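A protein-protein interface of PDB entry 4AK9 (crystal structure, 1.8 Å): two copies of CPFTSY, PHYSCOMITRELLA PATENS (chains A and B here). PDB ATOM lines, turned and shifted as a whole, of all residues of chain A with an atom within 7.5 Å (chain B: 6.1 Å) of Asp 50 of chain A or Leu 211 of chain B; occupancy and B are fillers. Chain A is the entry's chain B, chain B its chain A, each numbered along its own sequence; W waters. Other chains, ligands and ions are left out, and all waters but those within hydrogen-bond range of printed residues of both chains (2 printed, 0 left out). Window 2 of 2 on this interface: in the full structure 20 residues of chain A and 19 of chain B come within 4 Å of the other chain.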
ATOM      1  N   LEU A  36     -17.773  31.579  -8.522  1.00  0.00           N
ATOM      2  CA  LEU A  36     -19.219  31.571  -8.561  1.00  0.00           C
ATOM      3  C   LEU A  36     -19.836  30.995  -7.275  1.00  0.00           C
ATOM      4  O   LEU A  36     -20.835  31.530  -6.778  1.00  0.00           O
ATOM      5  CB  LEU A  36     -19.672  30.796  -9.804  1.00  0.00           C
ATOM      6  CG  LEU A  36     -21.119  30.790 -10.248  1.00  0.00           C
ATOM      7  CD1 LEU A  36     -21.609  32.213 -10.490  1.00  0.00           C
ATOM      8  CD2 LEU A  36     -21.227  29.950 -11.521  1.00  0.00           C
ATOM      9  N   SER A  45     -29.950  30.500  -5.084  1.00  0.00           N
ATOM     10  CA  SER A  45     -29.370  29.247  -5.596  1.00  0.00           C
ATOM     11  C   SER A  45     -29.655  29.007  -7.064  1.00  0.00           C
ATOM     12  O   SER A  45     -28.735  28.694  -7.824  1.00  0.00           O
ATOM     13  CB  SER A  45     -29.840  28.045  -4.765  1.00  0.00           C
ATOM     14  OG  SER A  45     -28.953  26.938  -4.889  1.00  0.00           O
ATOM     15  N   GLU A  46     -30.916  29.148  -7.455  1.00  0.00           N
ATOM     16  CA  GLU A  46     -31.321  28.860  -8.829  1.00  0.00           C
ATOM     17  C   GLU A  46     -30.608  29.732  -9.861  1.00  0.00           C
ATOM     18  O   GLU A  46     -30.240  29.245 -10.924  1.00  0.00           O
ATOM     19  CB  GLU A  46     -32.836  28.949  -8.981  1.00  0.00           C
ATOM     20  CG  GLU A  46     -33.590  27.872  -8.195  1.00  0.00           C
ATOM     21  CD  GLU A  46     -33.361  26.456  -8.721  1.00  0.00           C
ATOM     22  OE1 GLU A  46     -32.233  25.923  -8.571  1.00  0.00           O
ATOM     23  OE2 GLU A  46     -34.324  25.872  -9.271  1.00  0.00           O
ATOM     24  N   SER A  47     -30.402  31.006  -9.529  1.00  0.00           N
ATOM     25  CA  SER A  47     -29.630  31.909 -10.388  1.00  0.00           C
ATOM     26  C   SER A  47     -28.174  31.478 -10.497  1.00  0.00           C
ATOM     27  O   SER A  47     -27.579  31.525 -11.585  1.00  0.00           O
ATOM     28  CB  SER A  47     -29.675  33.344  -9.844  1.00  0.00           C
ATOM     29  OG  SER A  47     -30.984  33.885  -9.957  1.00  0.00           O
ATOM     30  N   ILE A  48     -27.596  31.087  -9.361  1.00  0.00           N
ATOM     31  CA  ILE A  48     -26.206  30.669  -9.331  1.00  0.00           C
ATOM     32  C   ILE A  48     -26.018  29.377 -10.122  1.00  0.00           C
ATOM     33  O   ILE A  48     -25.019  29.228 -10.830  1.00  0.00           O
ATOM     34  CB  ILE A  48     -25.700  30.501  -7.891  1.00  0.00           C
ATOM     35  CG1 ILE A  48     -25.684  31.860  -7.190  1.00  0.00           C
ATOM     36  CG2 ILE A  48     -24.300  29.934  -7.844  1.00  0.00           C
ATOM     37  CD1 ILE A  48     -25.186  32.996  -8.061  1.00  0.00           C
ATOM     38  N   LEU A  49     -26.987  28.467 -10.022  1.00  0.00           N
ATOM     39  CA  LEU A  49     -26.881  27.191 -10.741  1.00  0.00           C
ATOM     40  C   LEU A  49     -27.070  27.388 -12.244  1.00  0.00           C
ATOM     41  O   LEU A  49     -26.454  26.696 -13.036  1.00  0.00           O
ATOM     42  CB  LEU A  49     -27.857  26.158 -10.199  1.00  0.00           C
ATOM     43  CG  LEU A  49     -27.569  25.730  -8.748  1.00  0.00           C
ATOM     44  CD1 LEU A  49     -28.591  24.700  -8.281  1.00  0.00           C
ATOM     45  CD2 LEU A  49     -26.165  25.188  -8.595  1.00  0.00           C
ATOM     46  N   ASP A  50     -27.908  28.346 -12.631  1.00  0.00           N
ATOM     47  CA  ASP A  50     -28.017  28.705 -14.049  1.00  0.00           C
ATOM     48  C   ASP A  50     -26.676  29.200 -14.587  1.00  0.00           C
ATOM     49  O   ASP A  50     -26.233  28.794 -15.670  1.00  0.00           O
ATOM     50  CB  ASP A  50     -29.095  29.766 -14.257  1.00  0.00           C
ATOM     51  CG  ASP A  50     -30.485  29.169 -14.436  1.00  0.00           C
ATOM     52  OD1 ASP A  50     -30.676  27.944 -14.215  1.00  0.00           O
ATOM     53  OD2 ASP A  50     -31.405  29.943 -14.805  1.00  0.00           O
ATOM     54  N   GLU A  51     -26.026  30.074 -13.825  1.00  0.00           N
ATOM     55  CA  GLU A  51     -24.698  30.536 -14.209  1.00  0.00           C
ATOM     56  C   GLU A  51     -23.686  29.414 -14.225  1.00  0.00           C
ATOM     57  O   GLU A  51     -22.815  29.378 -15.090  1.00  0.00           O
ATOM     58  CB  GLU A  51     -24.216  31.616 -13.268  1.00  0.00           C
ATOM     59  CG  GLU A  51     -25.080  32.852 -13.315  1.00  0.00           C
ATOM     60  CD  GLU A  51     -24.534  33.950 -12.426  1.00  0.00           C
ATOM     61  OE1 GLU A  51     -23.307  34.216 -12.492  1.00  0.00           O
ATOM     62  OE2 GLU A  51     -25.334  34.535 -11.658  1.00  0.00           O
ATOM     63  N   LEU A  52     -23.783  28.506 -13.251  1.00  0.00           N
ATOM     64  CA  LEU A  52     -22.918  27.327 -13.252  1.00  0.00           C
ATOM     65  C   LEU A  52     -23.146  26.482 -14.513  1.00  0.00           C
ATOM     66  O   LEU A  52     -22.184  26.041 -15.175  1.00  0.00           O
ATOM     67  CB  LEU A  52     -23.175  26.476 -12.002  1.00  0.00           C
ATOM     68  CG  LEU A  52     -22.456  25.118 -11.986  1.00  0.00           C
ATOM     69  CD1 LEU A  52     -20.960  25.334 -11.984  1.00  0.00           C
ATOM     70  CD2 LEU A  52     -22.880  24.257 -10.785  1.00  0.00           C
ATOM     71  N   GLU A  53     -24.407  26.255 -14.854  1.00  0.00           N
ATOM     72  CA  GLU A  53     -24.679  25.451 -16.042  1.00  0.00           C
ATOM     73  C   GLU A  53     -24.123  26.137 -17.298  1.00  0.00           C
ATOM     74  O   GLU A  53     -23.557  25.476 -18.180  1.00  0.00           O
ATOM     75  CB  GLU A  53     -26.168  25.176 -16.191  1.00  0.00           C
ATOM     76  CG  GLU A  53     -26.464  23.951 -17.048  1.00  0.00           C
ATOM     77  CD  GLU A  53     -27.906  23.529 -16.950  1.00  0.00           C
ATOM     78  OE1 GLU A  53     -28.513  23.691 -15.854  1.00  0.00           O
ATOM     79  OE2 GLU A  53     -28.456  23.044 -17.967  1.00  0.00           O
ATOM     80  N   GLU A  54     -24.253  27.463 -17.370  1.00  0.00           N
ATOM     81  CA  GLU A  54     -23.667  28.191 -18.512  1.00  0.00           C
ATOM     82  C   GLU A  54     -22.143  28.125 -18.569  1.00  0.00           C
ATOM     83  O   GLU A  54     -21.567  28.039 -19.654  1.00  0.00           O
ATOM     84  CB  GLU A  54     -24.189  29.619 -18.573  1.00  0.00           C
ATOM     85  CG  GLU A  54     -25.686  29.662 -18.831  1.00  0.00           C
ATOM     86  CD  GLU A  54     -26.086  30.621 -19.961  1.00  0.00           C
ATOM     87  OE1 GLU A  54     -26.080  31.852 -19.713  1.00  0.00           O
ATOM     88  OE2 GLU A  54     -26.424  30.153 -21.089  1.00  0.00           O
ATOM     89  N   VAL A  55     -21.472  28.124 -17.413  1.00  0.00           N
ATOM     90  CA  VAL A  55     -20.033  27.899 -17.414  1.00  0.00           C
ATOM     91  C   VAL A  55     -19.697  26.560 -18.022  1.00  0.00           C
ATOM     92  O   VAL A  55     -18.769  26.471 -18.840  1.00  0.00           O
ATOM     93  CB  VAL A  55     -19.410  28.043 -16.001  1.00  0.00           C
ATOM     94  CG1 VAL A  55     -17.935  27.619 -16.003  1.00  0.00           C
ATOM     95  CG2 VAL A  55     -19.526  29.505 -15.553  1.00  0.00           C
ATOM     96  N   LEU A  56     -20.429  25.511 -17.632  1.00  0.00           N
ATOM     97  CA  LEU A  56     -20.225  24.193 -18.259  1.00  0.00           C
ATOM     98  C   LEU A  56     -20.443  24.221 -19.782  1.00  0.00           C
ATOM     99  O   LEU A  56     -19.695  23.564 -20.529  1.00  0.00           O
ATOM    100  CB  LEU A  56     -21.134  23.137 -17.639  1.00  0.00           C
ATOM    101  CG  LEU A  56     -20.987  22.908 -16.122  1.00  0.00           C
ATOM    102  CD1 LEU A  56     -21.871  21.735 -15.672  1.00  0.00           C
ATOM    103  CD2 LEU A  56     -19.497  22.707 -15.692  1.00  0.00           C
ATOM    104  N   LEU A  57     -21.477  24.936 -20.232  1.00  0.00           N
ATOM    105  CA  LEU A  57     -21.742  24.999 -21.685  1.00  0.00           C
ATOM    106  C   LEU A  57     -20.579  25.664 -22.436  1.00  0.00           C
ATOM    107  O   LEU A  57     -20.277  25.284 -23.566  1.00  0.00           O
ATOM    108  CB  LEU A  57     -23.061  25.703 -22.007  1.00  0.00           C
ATOM    109  CG  LEU A  57     -24.343  24.994 -21.514  1.00  0.00           C
ATOM    110  CD1 LEU A  57     -25.556  25.882 -21.859  1.00  0.00           C
ATOM    111  CD2 LEU A  57     -24.536  23.614 -22.114  1.00  0.00           C
ATOM    112  N   ALA A  66     -25.040  18.950 -19.448  1.00  0.00           N
ATOM    113  CA  ALA A  66     -24.953  20.017 -18.431  1.00  0.00           C
ATOM    114  C   ALA A  66     -26.263  20.057 -17.638  1.00  0.00           C
ATOM    115  O   ALA A  66     -26.268  20.242 -16.405  1.00  0.00           O
ATOM    116  CB  ALA A  66     -24.690  21.368 -19.076  1.00  0.00           C
ATOM    117  N   LEU A  67     -27.368  19.848 -18.345  1.00  0.00           N
ATOM    118  CA  LEU A  67     -28.690  19.792 -17.708  1.00  0.00           C
ATOM    119  C   LEU A  67     -28.726  18.720 -16.614  1.00  0.00           C
ATOM    120  O   LEU A  67     -29.090  19.013 -15.458  1.00  0.00           O
ATOM    121  CB  LEU A  67     -29.761  19.560 -18.782  1.00  0.00           C
ATOM    122  CG  LEU A  67     -31.190  19.246 -18.329  1.00  0.00           C
ATOM    123  CD1 LEU A  67     -31.645  20.230 -17.271  1.00  0.00           C
ATOM    124  CD2 LEU A  67     -32.088  19.310 -19.552  1.00  0.00           C
ATOM    125  N   VAL A  70     -26.362  19.449 -13.492  1.00  0.00           N
ATOM    126  CA  VAL A  70     -26.766  20.523 -12.604  1.00  0.00           C
ATOM    127  C   VAL A  70     -28.124  20.184 -11.957  1.00  0.00           C
ATOM    128  O   VAL A  70     -28.376  20.510 -10.792  1.00  0.00           O
ATOM    129  CB  VAL A  70     -26.738  21.904 -13.338  1.00  0.00           C
ATOM    130  CG1 VAL A  70     -27.361  22.993 -12.487  1.00  0.00           C
ATOM    131  CG2 VAL A  70     -25.293  22.298 -13.678  1.00  0.00           C
ATOM    132  N   ARG A  74     -29.203  20.377  -8.022  1.00  0.00           N
ATOM    133  CA  ARG A  74     -30.398  21.095  -7.565  1.00  0.00           C
ATOM    134  C   ARG A  74     -31.277  20.236  -6.622  1.00  0.00           C
ATOM    135  O   ARG A  74     -31.671  20.685  -5.517  1.00  0.00           O
ATOM    136  CB  ARG A  74     -31.196  21.582  -8.773  1.00  0.00           C
ATOM    137  CG  ARG A  74     -32.549  22.158  -8.438  1.00  0.00           C
ATOM    138  CD  ARG A  74     -33.222  22.805  -9.629  1.00  0.00           C
ATOM    139  NE  ARG A  74     -32.422  23.901 -10.187  1.00  0.00           N
ATOM    140  CZ  ARG A  74     -31.735  23.815 -11.327  1.00  0.00           C
ATOM    141  NH1 ARG A  74     -31.760  22.682 -12.027  1.00  0.00           N
ATOM    142  NH2 ARG A  74     -31.033  24.858 -11.765  1.00  0.00           N
ATOM    143  N   VAL B 124     -32.257  34.199 -21.300  1.00  0.00           N
ATOM    144  CA  VAL B 124     -32.051  33.509 -20.028  1.00  0.00           C
ATOM    145  C   VAL B 124     -31.310  34.344 -19.006  1.00  0.00           C
ATOM    146  O   VAL B 124     -31.516  34.192 -17.806  1.00  0.00           O
ATOM    147  CB  VAL B 124     -31.302  32.157 -20.203  1.00  0.00           C
ATOM    148  CG1 VAL B 124     -31.790  31.443 -21.443  1.00  0.00           C
ATOM    149  CG2 VAL B 124     -29.802  32.369 -20.265  1.00  0.00           C
ATOM    150  N   GLY B 209     -36.681  35.498 -17.387  1.00  0.00           N
ATOM    151  CA  GLY B 209     -36.356  34.299 -18.153  1.00  0.00           C
ATOM    152  C   GLY B 209     -35.332  33.466 -17.418  1.00  0.00           C
ATOM    153  O   GLY B 209     -34.566  34.008 -16.616  1.00  0.00           O
ATOM    154  N   ARG B 210     -35.357  32.159 -17.661  1.00  0.00           N
ATOM    155  CA  ARG B 210     -34.387  31.242 -17.094  1.00  0.00           C
ATOM    156  C   ARG B 210     -33.763  30.394 -18.200  1.00  0.00           C
ATOM    157  O   ARG B 210     -34.252  30.356 -19.321  1.00  0.00           O
ATOM    158  CB  ARG B 210     -35.066  30.311 -16.087  1.00  0.00           C
ATOM    159  CG  ARG B 210     -35.740  31.041 -14.924  1.00  0.00           C
ATOM    160  CD  ARG B 210     -34.779  31.285 -13.752  1.00  0.00           C
ATOM    161  NE  ARG B 210     -34.090  30.078 -13.254  1.00  0.00           N
ATOM    162  CZ  ARG B 210     -34.672  28.922 -12.896  1.00  0.00           C
ATOM    163  NH1 ARG B 210     -35.991  28.748 -12.979  1.00  0.00           N
ATOM    164  NH2 ARG B 210     -33.915  27.916 -12.448  1.00  0.00           N
ATOM    165  N   LEU B 211     -32.704  29.689 -17.847  1.00  0.00           N
ATOM    166  CA  LEU B 211     -32.038  28.800 -18.794  1.00  0.00           C
ATOM    167  C   LEU B 211     -32.959  27.698 -19.247  1.00  0.00           C
ATOM    168  O   LEU B 211     -32.988  27.342 -20.427  1.00  0.00           O
ATOM    169  CB  LEU B 211     -30.814  28.211 -18.130  1.00  0.00           C
ATOM    170  CG  LEU B 211     -29.967  27.337 -19.050  1.00  0.00           C
ATOM    171  CD1 LEU B 211     -29.605  28.090 -20.323  1.00  0.00           C
ATOM    172  CD2 LEU B 211     -28.732  26.958 -18.239  1.00  0.00           C
ATOM    173  N   HIS B 212     -33.740  27.161 -18.317  1.00  0.00           N
ATOM    174  CA  HIS B 212     -34.757  26.177 -18.677  1.00  0.00           C
ATOM    175  C   HIS B 212     -36.143  26.703 -18.325  1.00  0.00           C
ATOM    176  O   HIS B 212     -36.413  27.004 -17.165  1.00  0.00           O
ATOM    177  CB  HIS B 212     -34.459  24.857 -17.987  1.00  0.00           C
ATOM    178  CG  HIS B 212     -33.096  24.335 -18.320  1.00  0.00           C
ATOM    179  ND1 HIS B 212     -32.791  23.829 -19.560  1.00  0.00           N
ATOM    180  CD2 HIS B 212     -31.948  24.305 -17.598  1.00  0.00           C
ATOM    181  CE1 HIS B 212     -31.512  23.479 -19.585  1.00  0.00           C
ATOM    182  NE2 HIS B 212     -30.984  23.752 -18.409  1.00  0.00           N
ATOM    183  N   THR B 213     -36.998  26.826 -19.342  1.00  0.00           N
ATOM    184  CA  THR B 213     -38.369  27.294 -19.152  1.00  0.00           C
ATOM    185  C   THR B 213     -39.196  26.251 -18.434  1.00  0.00           C
ATOM    186  O   THR B 213     -39.058  25.048 -18.679  1.00  0.00           O
ATOM    187  CB  THR B 213     -39.048  27.664 -20.511  1.00  0.00           C
ATOM    188  OG1 THR B 213     -40.346  28.242 -20.279  1.00  0.00           O
ATOM    189  CG2 THR B 213     -39.177  26.441 -21.451  1.00  0.00           C
ATOM    190  N   GLN B 254     -31.487  26.857 -26.196  1.00  0.00           N
ATOM    191  CA  GLN B 254     -32.338  27.863 -25.566  1.00  0.00           C
ATOM    192  C   GLN B 254     -33.020  28.757 -26.626  1.00  0.00           C
ATOM    193  O   GLN B 254     -34.126  29.259 -26.399  1.00  0.00           O
ATOM    194  CB  GLN B 254     -31.553  28.678 -24.521  1.00  0.00           C
ATOM    195  CG  GLN B 254     -30.515  29.555 -25.121  1.00  0.00           C
ATOM    196  CD  GLN B 254     -29.595  30.141 -24.085  1.00  0.00           C
ATOM    197  OE1 GLN B 254     -29.643  31.341 -23.825  1.00  0.00           O
ATOM    198  NE2 GLN B 254     -28.736  29.297 -23.485  1.00  0.00           N
ATOM    199  N   GLU B 257     -36.142  26.892 -27.730  1.00  0.00           N
ATOM    200  CA  GLU B 257     -37.105  26.894 -26.633  1.00  0.00           C
ATOM    201  C   GLU B 257     -37.813  28.232 -26.533  1.00  0.00           C
ATOM    202  O   GLU B 257     -39.052  28.274 -26.448  1.00  0.00           O
ATOM    203  CB  GLU B 257     -36.420  26.556 -25.307  1.00  0.00           C
ATOM    204  CG  GLU B 257     -35.977  25.097 -25.214  1.00  0.00           C
ATOM    205  CD  GLU B 257     -35.036  24.819 -24.033  1.00  0.00           C
ATOM    206  OE1 GLU B 257     -35.286  25.373 -22.929  1.00  0.00           O
ATOM    207  OE2 GLU B 257     -34.064  24.035 -24.213  1.00  0.00           O
ATOM    208  N   PHE B 258     -37.055  29.328 -26.552  1.00  0.00           N
ATOM    209  CA  PHE B 258     -37.701  30.643 -26.470  1.00  0.00           C
ATOM    210  C   PHE B 258     -38.623  30.923 -27.644  1.00  0.00           C
ATOM    211  O   PHE B 258     -39.691  31.518 -27.489  1.00  0.00           O
ATOM    212  CB  PHE B 258     -36.669  31.787 -26.283  1.00  0.00           C
ATOM    213  CG  PHE B 258     -36.338  32.067 -24.851  1.00  0.00           C
ATOM    214  CD1 PHE B 258     -35.418  31.274 -24.161  1.00  0.00           C
ATOM    215  CD2 PHE B 258     -36.987  33.084 -24.161  1.00  0.00           C
ATOM    216  CE1 PHE B 258     -35.122  31.507 -22.825  1.00  0.00           C
ATOM    217  CE2 PHE B 258     -36.692  33.318 -22.816  1.00  0.00           C
ATOM    218  CZ  PHE B 258     -35.764  32.532 -22.144  1.00  0.00           C
HETATM  219  O   HOH W   1     -33.232  27.094 -15.400  1.00  0.00           O
HETATM  220  O   HOH W   2     -32.866  25.030 -14.069  1.00  0.00           O
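No position is printed for both chains.
Of the 9 pairs that touch across the chains among the printed residues, none has its exchanged pair printed and touching as well.
Water W1 lies within hydrogen-bond range of the side-chain carboxylate (OD1) of Asp 50 of chain A, the backbone NH (N) of His 212 of chain B and the guanidinium group (NH2) of Arg 210 of chain B.
Water W2 bridges NH2 of Arg 74 of chain A and NH2 of Arg 210 of chain B.
NH2 of Arg 210 of chain B lies within salt-bridge range of OE2 of Glu 46 of chain A.
NE of Arg 210 of chain B lies within salt-bridge range of OD2 of Asp 50 of chain A, 3.1 Å away.
A ring nitrogen (NE2) of His 212 of chain B sits at hydrogen-bond distance from the side-chain carboxylate of Glu 53 of chain A (2.7 Å).
The backbone NH of Leu 211 of chain B sits at hydrogen-bond distance from the side-chain carboxylate of Asp 50 of chain A, at 3.3 Å.
The side-chain carboxylate (OE2) of Glu 54 of chain A is in hydrogen-bond range of the side-chain amide nitrogen (NE2) of Gln 254 of chain B, 3.4 Å away.
Of the 9 printed residues of chain B, 5 touch a printed residue of chain A.
Hydrophobic or aromatic side chains of chain B within 4 Å of the printed part of chain A: Val 124, Leu 211 and His 212.
Among the printed residues, Asp or Glu carboxylates within 4 Å of a Lys or Arg side-chain nitrogen of the other chain: Glu 46 of chain A with Arg 210 of chain B (3.8 Å) and Asp 50 of chain A with Arg 210 of chain B (3.1 Å).
OE2 of Glu 53 of chain A sits close to N of Leu 67 of chain A, at 3.4 Å.
The side-chain carboxylate (OD1) of Asp 50 of chain A lies within salt-bridge range of the guanidinium group (NH2) of Arg 74 of chain A (3.96 Å).
The side-chain carboxylate (OE1) of Glu 46 of chain A lies within salt-bridge range of the guanidinium group (NE) of Arg 74 of chain A, 2.6 Å away.
Among the printed residues, merely in contact across the chains: Glu 53 of chain A with Leu 211 of chain B (3.7 Å), Glu 54 of chain A with Val 124 of chain B (3.8 Å), Glu 54 of chain A with Leu 211 of chain B (3.9 Å) and Leu 67 of chain A with His 212 of chain B (3.8 Å).
Of chain B, only Arg 210 (3.1 Å) and Leu 211 (3.3 Å) come within 4 Å of Asp 50 of chain A.
Leu 211 of chain B touches just these residues of chain A: Asp 50 (3.3 Å), Glu 53 (3.7 Å) and Glu 54 (3.9 Å).
Of the printed residues of chain A, His 212 of chain B touches Glu 53 (2.7 Å) and Leu 67 (3.8 Å).
Printed residues of chain A within 4 Å of Gln 254 of chain B: Glu 54.
The nearest residue of chain B that does not touch Asp 50 of chain A is His 212 of chain B (5.1 Å).
The nearest residue of chain A that does not touch Leu 211 of chain B is Leu 57 of chain A (4.9 Å).
The nearest printed residue of chain B that does not touch Glu 53 of chain A is Arg 210 of chain B (7.7 Å).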
